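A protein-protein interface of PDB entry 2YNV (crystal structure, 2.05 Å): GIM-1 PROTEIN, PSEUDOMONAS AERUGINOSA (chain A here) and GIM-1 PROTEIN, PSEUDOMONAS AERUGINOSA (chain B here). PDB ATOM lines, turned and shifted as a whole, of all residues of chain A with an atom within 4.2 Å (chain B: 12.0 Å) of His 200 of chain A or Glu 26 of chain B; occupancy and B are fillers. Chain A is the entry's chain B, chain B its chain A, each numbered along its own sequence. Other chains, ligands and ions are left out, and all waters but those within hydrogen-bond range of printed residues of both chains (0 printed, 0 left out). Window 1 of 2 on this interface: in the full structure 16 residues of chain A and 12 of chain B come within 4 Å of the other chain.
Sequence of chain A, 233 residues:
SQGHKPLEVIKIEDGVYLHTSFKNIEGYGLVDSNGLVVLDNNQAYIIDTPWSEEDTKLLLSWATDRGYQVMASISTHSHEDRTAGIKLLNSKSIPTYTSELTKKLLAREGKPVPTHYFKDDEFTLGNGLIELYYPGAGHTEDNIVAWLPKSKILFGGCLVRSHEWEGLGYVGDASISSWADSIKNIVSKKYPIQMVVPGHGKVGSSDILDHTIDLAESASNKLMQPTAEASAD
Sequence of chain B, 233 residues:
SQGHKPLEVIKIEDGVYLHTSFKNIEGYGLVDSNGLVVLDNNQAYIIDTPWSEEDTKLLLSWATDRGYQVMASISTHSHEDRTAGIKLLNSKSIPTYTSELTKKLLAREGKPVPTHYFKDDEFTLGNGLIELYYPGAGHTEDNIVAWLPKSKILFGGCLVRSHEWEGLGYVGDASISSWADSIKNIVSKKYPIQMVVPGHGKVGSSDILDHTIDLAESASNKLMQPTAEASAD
Of the printed residues of chain B, His 200 of chain A touches Glu 26 (3.7 Å). Glu 26 of chain B touches three residues of chain A. No residue of chain B comes within 4 Å of Ser 33 of chain A. Asn 34 of chain A touches none of the printed residues of chain B. Trp 51 of chain A touches just one residue of chain B: Glu 26. Asp 81 of chain A touches one residue of chain B. No residue of chain B comes within 4 Å of Ser 162 of chain A. No residue of chain B comes within 4 Å of Gly 199 of chain A. No residue of chain B comes within 4 Å of Gly 201 of chain A. Gly 29 of chain B touches none of the printed residues of chain A. The nearest residue of chain B that does not touch His 200 of chain A is Gly 27 of chain B (4.3 Å).
The side-chain carboxylate of Glu 26 of chain B sits at hydrogen-bond distance from the indole nitrogen of Trp 51 of chain A.
Among the printed residues, pairs that only touch across the chains: Asp 81 of chain A with Glu 26 of chain B and His 200 of chain A with Glu 26 of chain B.
ND1 of His 200 of chain A sits at hydrogen-bond distance from O of Asp 32 of chain A, at 2.7 Å. The side-chain carboxylate (OD2) of Asp 81 of chain A lies within salt-bridge range of the guanidinium group (NE) of Arg 82 of chain A (3.2 Å). OD2 of Asp 81 of chain A lies within hydrogen-bond range of NE2 of His 200 of chain A, at 3.5 Å. NE2 of His 200 of chain A is in hydrogen-bond range of SG of Cys 158 of chain A (3.0 Å).
Hydrophobic or aromatic side chains of chain A within 4 Å of the printed part of chain B: Trp 51 and His 200.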
ATOM      1  N   ASP A  32     -18.083   6.675  28.638  1.00  0.00           N
ATOM      2  CA  ASP A  32     -16.984   6.023  29.323  1.00  0.00           C
ATOM      3  C   ASP A  32     -16.220   5.151  28.336  1.00  0.00           C
ATOM      4  O   ASP A  32     -16.822   4.570  27.426  1.00  0.00           O
ATOM      5  CB  ASP A  32     -17.502   5.158  30.476  1.00  0.00           C
ATOM      6  CG  ASP A  32     -18.126   3.858  30.008  1.00  0.00           C
ATOM      7  OD1 ASP A  32     -17.414   2.837  29.843  1.00  0.00           O
ATOM      8  OD2 ASP A  32     -19.358   3.848  29.831  1.00  0.00           O
ATOM      9  N   SER A  33     -14.899   5.079  28.534  1.00  0.00           N
ATOM     10  CA  SER A  33     -14.006   4.188  27.798  1.00  0.00           C
ATOM     11  C   SER A  33     -12.975   3.511  28.755  1.00  0.00           C
ATOM     12  O   SER A  33     -12.488   4.161  29.689  1.00  0.00           O
ATOM     13  CB  SER A  33     -13.265   4.969  26.735  1.00  0.00           C
ATOM     14  OG  SER A  33     -12.123   4.228  26.296  1.00  0.00           O
ATOM     15  N   ASN A  34     -12.681   2.227  28.500  1.00  0.00           N
ATOM     16  CA  ASN A  34     -11.843   1.395  29.360  1.00  0.00           C
ATOM     17  C   ASN A  34     -10.525   0.974  28.681  1.00  0.00           C
ATOM     18  O   ASN A  34     -10.496   0.649  27.487  1.00  0.00           O
ATOM     19  CB  ASN A  34     -12.528   0.062  29.728  1.00  0.00           C
ATOM     20  CG  ASN A  34     -13.863   0.228  30.431  1.00  0.00           C
ATOM     21  OD1 ASN A  34     -14.017   1.044  31.310  1.00  0.00           O
ATOM     22  ND2 ASN A  34     -14.824  -0.583  30.032  1.00  0.00           N
ATOM     23  N   TRP A  51      -8.826   8.420  26.752  1.00  0.00           N
ATOM     24  CA  TRP A  51      -9.285   9.362  25.740  1.00  0.00           C
ATOM     25  C   TRP A  51      -8.438  10.617  25.540  1.00  0.00           C
ATOM     26  O   TRP A  51      -8.081  10.990  24.426  1.00  0.00           O
ATOM     27  CB  TRP A  51     -10.679   9.814  26.137  1.00  0.00           C
ATOM     28  CG  TRP A  51     -11.699   9.459  25.164  1.00  0.00           C
ATOM     29  CD1 TRP A  51     -11.669   9.704  23.825  1.00  0.00           C
ATOM     30  CD2 TRP A  51     -12.944   8.804  25.433  1.00  0.00           C
ATOM     31  NE1 TRP A  51     -12.825   9.238  23.232  1.00  0.00           N
ATOM     32  CE2 TRP A  51     -13.621   8.674  24.202  1.00  0.00           C
ATOM     33  CE3 TRP A  51     -13.553   8.310  26.598  1.00  0.00           C
ATOM     34  CZ2 TRP A  51     -14.878   8.070  24.098  1.00  0.00           C
ATOM     35  CZ3 TRP A  51     -14.799   7.705  26.496  1.00  0.00           C
ATOM     36  CH2 TRP A  51     -15.448   7.590  25.255  1.00  0.00           C
ATOM     37  N   ASP A  81     -10.050   7.076  21.318  1.00  0.00           N
ATOM     38  CA  ASP A  81     -10.298   6.461  22.641  1.00  0.00           C
ATOM     39  C   ASP A  81      -9.215   5.418  23.015  1.00  0.00           C
ATOM     40  O   ASP A  81      -8.914   5.193  24.203  1.00  0.00           O
ATOM     41  CB  ASP A  81     -11.703   5.824  22.735  1.00  0.00           C
ATOM     42  CG  ASP A  81     -12.077   5.014  21.499  1.00  0.00           C
ATOM     43  OD1 ASP A  81     -11.646   5.385  20.386  1.00  0.00           O
ATOM     44  OD2 ASP A  81     -12.817   4.013  21.640  1.00  0.00           O
ATOM     45  N   ARG A  82      -8.655   4.790  21.982  1.00  0.00           N
ATOM     46  CA  ARG A  82      -7.532   3.896  22.123  1.00  0.00           C
ATOM     47  C   ARG A  82      -6.184   4.665  22.007  1.00  0.00           C
ATOM     48  O   ARG A  82      -5.173   4.219  22.582  1.00  0.00           O
ATOM     49  CB  ARG A  82      -7.591   2.800  21.045  1.00  0.00           C
ATOM     50  CG  ARG A  82      -8.985   2.252  20.710  1.00  0.00           C
ATOM     51  CD  ARG A  82      -9.593   1.271  21.752  1.00  0.00           C
ATOM     52  NE  ARG A  82     -10.680   1.859  22.544  1.00  0.00           N
ATOM     53  CZ  ARG A  82     -11.032   1.478  23.776  1.00  0.00           C
ATOM     54  NH1 ARG A  82     -10.401   0.493  24.402  1.00  0.00           N
ATOM     55  NH2 ARG A  82     -12.033   2.096  24.398  1.00  0.00           N
ATOM     56  N   CYS A 158     -13.230  -2.164  21.269  1.00  0.00           N
ATOM     57  CA  CYS A 158     -14.532  -1.883  20.654  1.00  0.00           C
ATOM     58  C   CYS A 158     -14.891  -2.929  19.622  1.00  0.00           C
ATOM     59  O   CYS A 158     -15.938  -2.825  18.971  1.00  0.00           O
ATOM     60  CB  CYS A 158     -14.586  -0.479  20.061  1.00  0.00           C
ATOM     61  SG  CYS A 158     -14.850   0.816  21.328  1.00  0.00           S
ATOM     62  N   SER A 162     -20.518  -4.618  25.551  1.00  0.00           N
ATOM     63  CA  SER A 162     -20.972  -5.128  26.829  1.00  0.00           C
ATOM     64  C   SER A 162     -22.448  -5.461  26.744  1.00  0.00           C
ATOM     65  O   SER A 162     -23.153  -4.996  25.849  1.00  0.00           O
ATOM     66  CB  SER A 162     -20.752  -4.093  27.925  1.00  0.00           C
ATOM     67  OG  SER A 162     -21.618  -2.986  27.731  1.00  0.00           O
ATOM     68  N   PRO A 198     -14.717  -4.881  27.746  1.00  0.00           N
ATOM     69  CA  PRO A 198     -15.058  -4.202  26.503  1.00  0.00           C
ATOM     70  C   PRO A 198     -14.426  -2.823  26.496  1.00  0.00           C
ATOM     71  O   PRO A 198     -13.990  -2.360  27.557  1.00  0.00           O
ATOM     72  CB  PRO A 198     -16.569  -4.058  26.628  1.00  0.00           C
ATOM     73  CG  PRO A 198     -16.732  -3.693  28.075  1.00  0.00           C
ATOM     74  CD  PRO A 198     -15.693  -4.560  28.807  1.00  0.00           C
ATOM     75  N   GLY A 199     -14.394  -2.162  25.350  1.00  0.00           N
ATOM     76  CA  GLY A 199     -13.853  -0.815  25.278  1.00  0.00           C
ATOM     77  C   GLY A 199     -14.710   0.216  26.011  1.00  0.00           C
ATOM     78  O   GLY A 199     -14.205   1.297  26.354  1.00  0.00           O
ATOM     79  N   HIS A 200     -15.988  -0.135  26.220  1.00  0.00           N
ATOM     80  CA  HIS A 200     -17.041   0.734  26.776  1.00  0.00           C
ATOM     81  C   HIS A 200     -17.984  -0.175  27.534  1.00  0.00           C
ATOM     82  O   HIS A 200     -18.360  -1.237  27.034  1.00  0.00           O
ATOM     83  CB  HIS A 200     -17.882   1.456  25.675  1.00  0.00           C
ATOM     84  CG  HIS A 200     -17.051   2.252  24.713  1.00  0.00           C
ATOM     85  ND1 HIS A 200     -16.521   3.489  25.024  1.00  0.00           N
ATOM     86  CD2 HIS A 200     -16.604   1.957  23.468  1.00  0.00           C
ATOM     87  CE1 HIS A 200     -15.779   3.918  24.016  1.00  0.00           C
ATOM     88  NE2 HIS A 200     -15.819   3.009  23.057  1.00  0.00           N
ATOM     89  N   GLY A 201     -18.361   0.238  28.740  1.00  0.00           N
ATOM     90  CA  GLY A 201     -19.404  -0.444  29.471  1.00  0.00           C
ATOM     91  C   GLY A 201     -18.786  -1.386  30.455  1.00  0.00           C
ATOM     92  O   GLY A 201     -17.644  -1.192  30.815  1.00  0.00           O
ATOM     93  N   LYS A 202     -19.496  -2.436  30.837  1.00  0.00           N
ATOM     94  CA  LYS A 202     -19.100  -3.225  31.996  1.00  0.00           C
ATOM     95  C   LYS A 202     -18.411  -4.526  31.622  1.00  0.00           C
ATOM     96  O   LYS A 202     -18.736  -5.167  30.619  1.00  0.00           O
ATOM     97  CB  LYS A 202     -20.321  -3.524  32.868  1.00  0.00           C
ATOM     98  CG  LYS A 202     -20.308  -2.840  34.216  1.00  0.00           C
ATOM     99  CD  LYS A 202     -21.630  -3.101  34.966  1.00  0.00           C
ATOM    100  CE  LYS A 202     -22.170  -1.840  35.642  1.00  0.00           C
ATOM    101  NZ  LYS A 202     -23.672  -1.836  35.732  1.00  0.00           N
ATOM    102  N   PHE B  22     -24.846  16.128  12.434  1.00  0.00           N
ATOM    103  CA  PHE B  22     -24.507  14.853  13.034  1.00  0.00           C
ATOM    104  C   PHE B  22     -23.088  14.889  13.569  1.00  0.00           C
ATOM    105  O   PHE B  22     -22.214  15.514  12.963  1.00  0.00           O
ATOM    106  CB  PHE B  22     -24.691  13.717  12.003  1.00  0.00           C
ATOM    107  CG  PHE B  22     -26.092  13.644  11.463  1.00  0.00           C
ATOM    108  CD1 PHE B  22     -26.463  14.403  10.365  1.00  0.00           C
ATOM    109  CD2 PHE B  22     -27.046  12.874  12.078  1.00  0.00           C
ATOM    110  CE1 PHE B  22     -27.741  14.371   9.894  1.00  0.00           C
ATOM    111  CE2 PHE B  22     -28.319  12.810  11.588  1.00  0.00           C
ATOM    112  CZ  PHE B  22     -28.669  13.573  10.497  1.00  0.00           C
ATOM    113  N   LYS B  23     -22.893  14.273  14.733  1.00  0.00           N
ATOM    114  CA  LYS B  23     -21.559  13.918  15.215  1.00  0.00           C
ATOM    115  C   LYS B  23     -21.517  12.427  15.573  1.00  0.00           C
ATOM    116  O   LYS B  23     -22.455  11.874  16.136  1.00  0.00           O
ATOM    117  CB  LYS B  23     -21.129  14.779  16.406  1.00  0.00           C
ATOM    118  CG  LYS B  23     -19.724  14.463  16.890  1.00  0.00           C
ATOM    119  N   ASN B  24     -20.390  11.810  15.304  1.00  0.00           N
ATOM    120  CA  ASN B  24     -20.290  10.381  15.458  1.00  0.00           C
ATOM    121  C   ASN B  24     -19.473   9.955  16.683  1.00  0.00           C
ATOM    122  O   ASN B  24     -18.296  10.291  16.783  1.00  0.00           O
ATOM    123  CB  ASN B  24     -19.678   9.848  14.185  1.00  0.00           C
ATOM    124  CG  ASN B  24     -18.946   8.560  14.391  1.00  0.00           C
ATOM    125  OD1 ASN B  24     -19.392   7.655  15.105  1.00  0.00           O
ATOM    126  ND2 ASN B  24     -17.774   8.488  13.791  1.00  0.00           N
ATOM    127  N   ILE B  25     -20.099   9.198  17.588  1.00  0.00           N
ATOM    128  CA  ILE B  25     -19.472   8.833  18.884  1.00  0.00           C
ATOM    129  C   ILE B  25     -18.861   7.429  19.015  1.00  0.00           C
ATOM    130  O   ILE B  25     -19.528   6.420  18.766  1.00  0.00           O
ATOM    131  CB  ILE B  25     -20.485   8.865  20.045  1.00  0.00           C
ATOM    132  CG1 ILE B  25     -20.760  10.277  20.528  1.00  0.00           C
ATOM    133  CG2 ILE B  25     -19.903   8.113  21.240  1.00  0.00           C
ATOM    134  CD1 ILE B  25     -21.021  11.234  19.454  1.00  0.00           C
ATOM    135  N   GLU B  26     -17.614   7.391  19.492  1.00  0.00           N
ATOM    136  CA  GLU B  26     -16.937   6.169  19.957  1.00  0.00           C
ATOM    137  C   GLU B  26     -17.854   5.009  20.331  1.00  0.00           C
ATOM    138  O   GLU B  26     -18.446   5.008  21.415  1.00  0.00           O
ATOM    139  CB  GLU B  26     -16.159   6.493  21.225  1.00  0.00           C
ATOM    140  CG  GLU B  26     -14.731   6.928  21.023  1.00  0.00           C
ATOM    141  CD  GLU B  26     -14.626   8.413  20.674  1.00  0.00           C
ATOM    142  OE1 GLU B  26     -15.663   9.106  20.734  1.00  0.00           O
ATOM    143  OE2 GLU B  26     -13.506   8.895  20.362  1.00  0.00           O
ATOM    144  N   GLY B  27     -17.984   4.030  19.443  1.00  0.00           N
ATOM    145  CA  GLY B  27     -18.662   2.778  19.771  1.00  0.00           C
ATOM    146  C   GLY B  27     -20.115   2.918  20.219  1.00  0.00           C
ATOM    147  O   GLY B  27     -20.757   1.921  20.579  1.00  0.00           O
ATOM    148  N   TYR B  28     -20.632   4.149  20.159  1.00  0.00           N
ATOM    149  CA  TYR B  28     -22.017   4.444  20.520  1.00  0.00           C
ATOM    150  C   TYR B  28     -22.853   4.680  19.268  1.00  0.00           C
ATOM    151  O   TYR B  28     -23.910   4.090  19.088  1.00  0.00           O
ATOM    152  CB  TYR B  28     -22.116   5.696  21.384  1.00  0.00           C
ATOM    153  CG  TYR B  28     -23.551   6.180  21.452  1.00  0.00           C
ATOM    154  CD1 TYR B  28     -24.101   6.939  20.420  1.00  0.00           C
ATOM    155  CD2 TYR B  28     -24.379   5.818  22.504  1.00  0.00           C
ATOM    156  CE1 TYR B  28     -25.424   7.346  20.457  1.00  0.00           C
ATOM    157  CE2 TYR B  28     -25.705   6.229  22.547  1.00  0.00           C
ATOM    158  CZ  TYR B  28     -26.220   6.988  21.521  1.00  0.00           C
ATOM    159  OH  TYR B  28     -27.535   7.407  21.558  1.00  0.00           O
ATOM    160  N   GLY B  29     -22.381   5.601  18.434  1.00  0.00           N
ATOM    161  CA  GLY B  29     -22.914   5.782  17.106  1.00  0.00           C
ATOM    162  C   GLY B  29     -23.172   7.235  16.805  1.00  0.00           C
ATOM    163  O   GLY B  29     -22.496   8.108  17.322  1.00  0.00           O
ATOM    164  N   LEU B  30     -24.185   7.458  15.982  1.00  0.00           N
ATOM    165  CA  LEU B  30     -24.485   8.754  15.424  1.00  0.00           C
ATOM    166  C   LEU B  30     -25.404   9.470  16.358  1.00  0.00           C
ATOM    167  O   LEU B  30     -26.428   8.959  16.771  1.00  0.00           O
ATOM    168  CB  LEU B  30     -25.222   8.599  14.109  1.00  0.00           C
ATOM    169  CG  LEU B  30     -24.581   9.032  12.795  1.00  0.00           C
ATOM    170  CD1 LEU B  30     -25.676   9.100  11.725  1.00  0.00           C
ATOM    171  CD2 LEU B  30     -23.883  10.361  12.907  1.00  0.00           C
ATOM    172  N   VAL B  31     -25.047  10.690  16.663  1.00  0.00           N
ATOM    173  CA  VAL B  31     -25.911  11.545  17.433  1.00  0.00           C
ATOM    174  C   VAL B  31     -26.265  12.728  16.515  1.00  0.00           C
ATOM    175  O   VAL B  31     -25.422  13.229  15.753  1.00  0.00           O
ATOM    176  CB  VAL B  31     -25.163  11.943  18.708  1.00  0.00           C
ATOM    177  CG1 VAL B  31     -24.574  10.706  19.307  1.00  0.00           C
ATOM    178  CG2 VAL B  31     -24.005  12.899  18.425  1.00  0.00           C
ATOM    179  N   ASP B  32     -27.523  13.130  16.531  1.00  0.00           N
ATOM    180  CA  ASP B  32     -27.959  14.240  15.709  1.00  0.00           C
ATOM    181  C   ASP B  32     -28.195  15.426  16.658  1.00  0.00           C
ATOM    182  O   ASP B  32     -28.214  15.237  17.891  1.00  0.00           O
ATOM    183  CB  ASP B  32     -29.245  13.834  15.072  1.00  0.00           C
ATOM    184  CG  ASP B  32     -30.350  13.765  16.088  1.00  0.00           C
ATOM    185  OD1 ASP B  32     -30.323  14.628  16.993  1.00  0.00           O
ATOM    186  OD2 ASP B  32     -31.202  12.875  16.022  1.00  0.00           O
ATOM    187  N   TRP B  51     -23.849  22.087  14.720  1.00  0.00           N
ATOM    188  CA  TRP B  51     -22.976  21.627  15.768  1.00  0.00           C
ATOM    189  C   TRP B  51     -21.503  21.926  15.453  1.00  0.00           C
ATOM    190  O   TRP B  51     -20.627  21.669  16.263  1.00  0.00           O
ATOM    191  CB  TRP B  51     -23.201  20.130  15.880  1.00  0.00           C
ATOM    192  CG  TRP B  51     -22.934  19.540  17.188  1.00  0.00           C
ATOM    193  CD1 TRP B  51     -22.129  20.038  18.191  1.00  0.00           C
ATOM    194  CD2 TRP B  51     -23.458  18.297  17.671  1.00  0.00           C
ATOM    195  NE1 TRP B  51     -22.120  19.165  19.263  1.00  0.00           N
ATOM    196  CE2 TRP B  51     -22.927  18.092  18.972  1.00  0.00           C
ATOM    197  CE3 TRP B  51     -24.320  17.335  17.132  1.00  0.00           C
ATOM    198  CZ2 TRP B  51     -23.254  16.969  19.741  1.00  0.00           C
ATOM    199  CZ3 TRP B  51     -24.637  16.219  17.888  1.00  0.00           C
ATOM    200  CH2 TRP B  51     -24.108  16.044  19.182  1.00  0.00           C
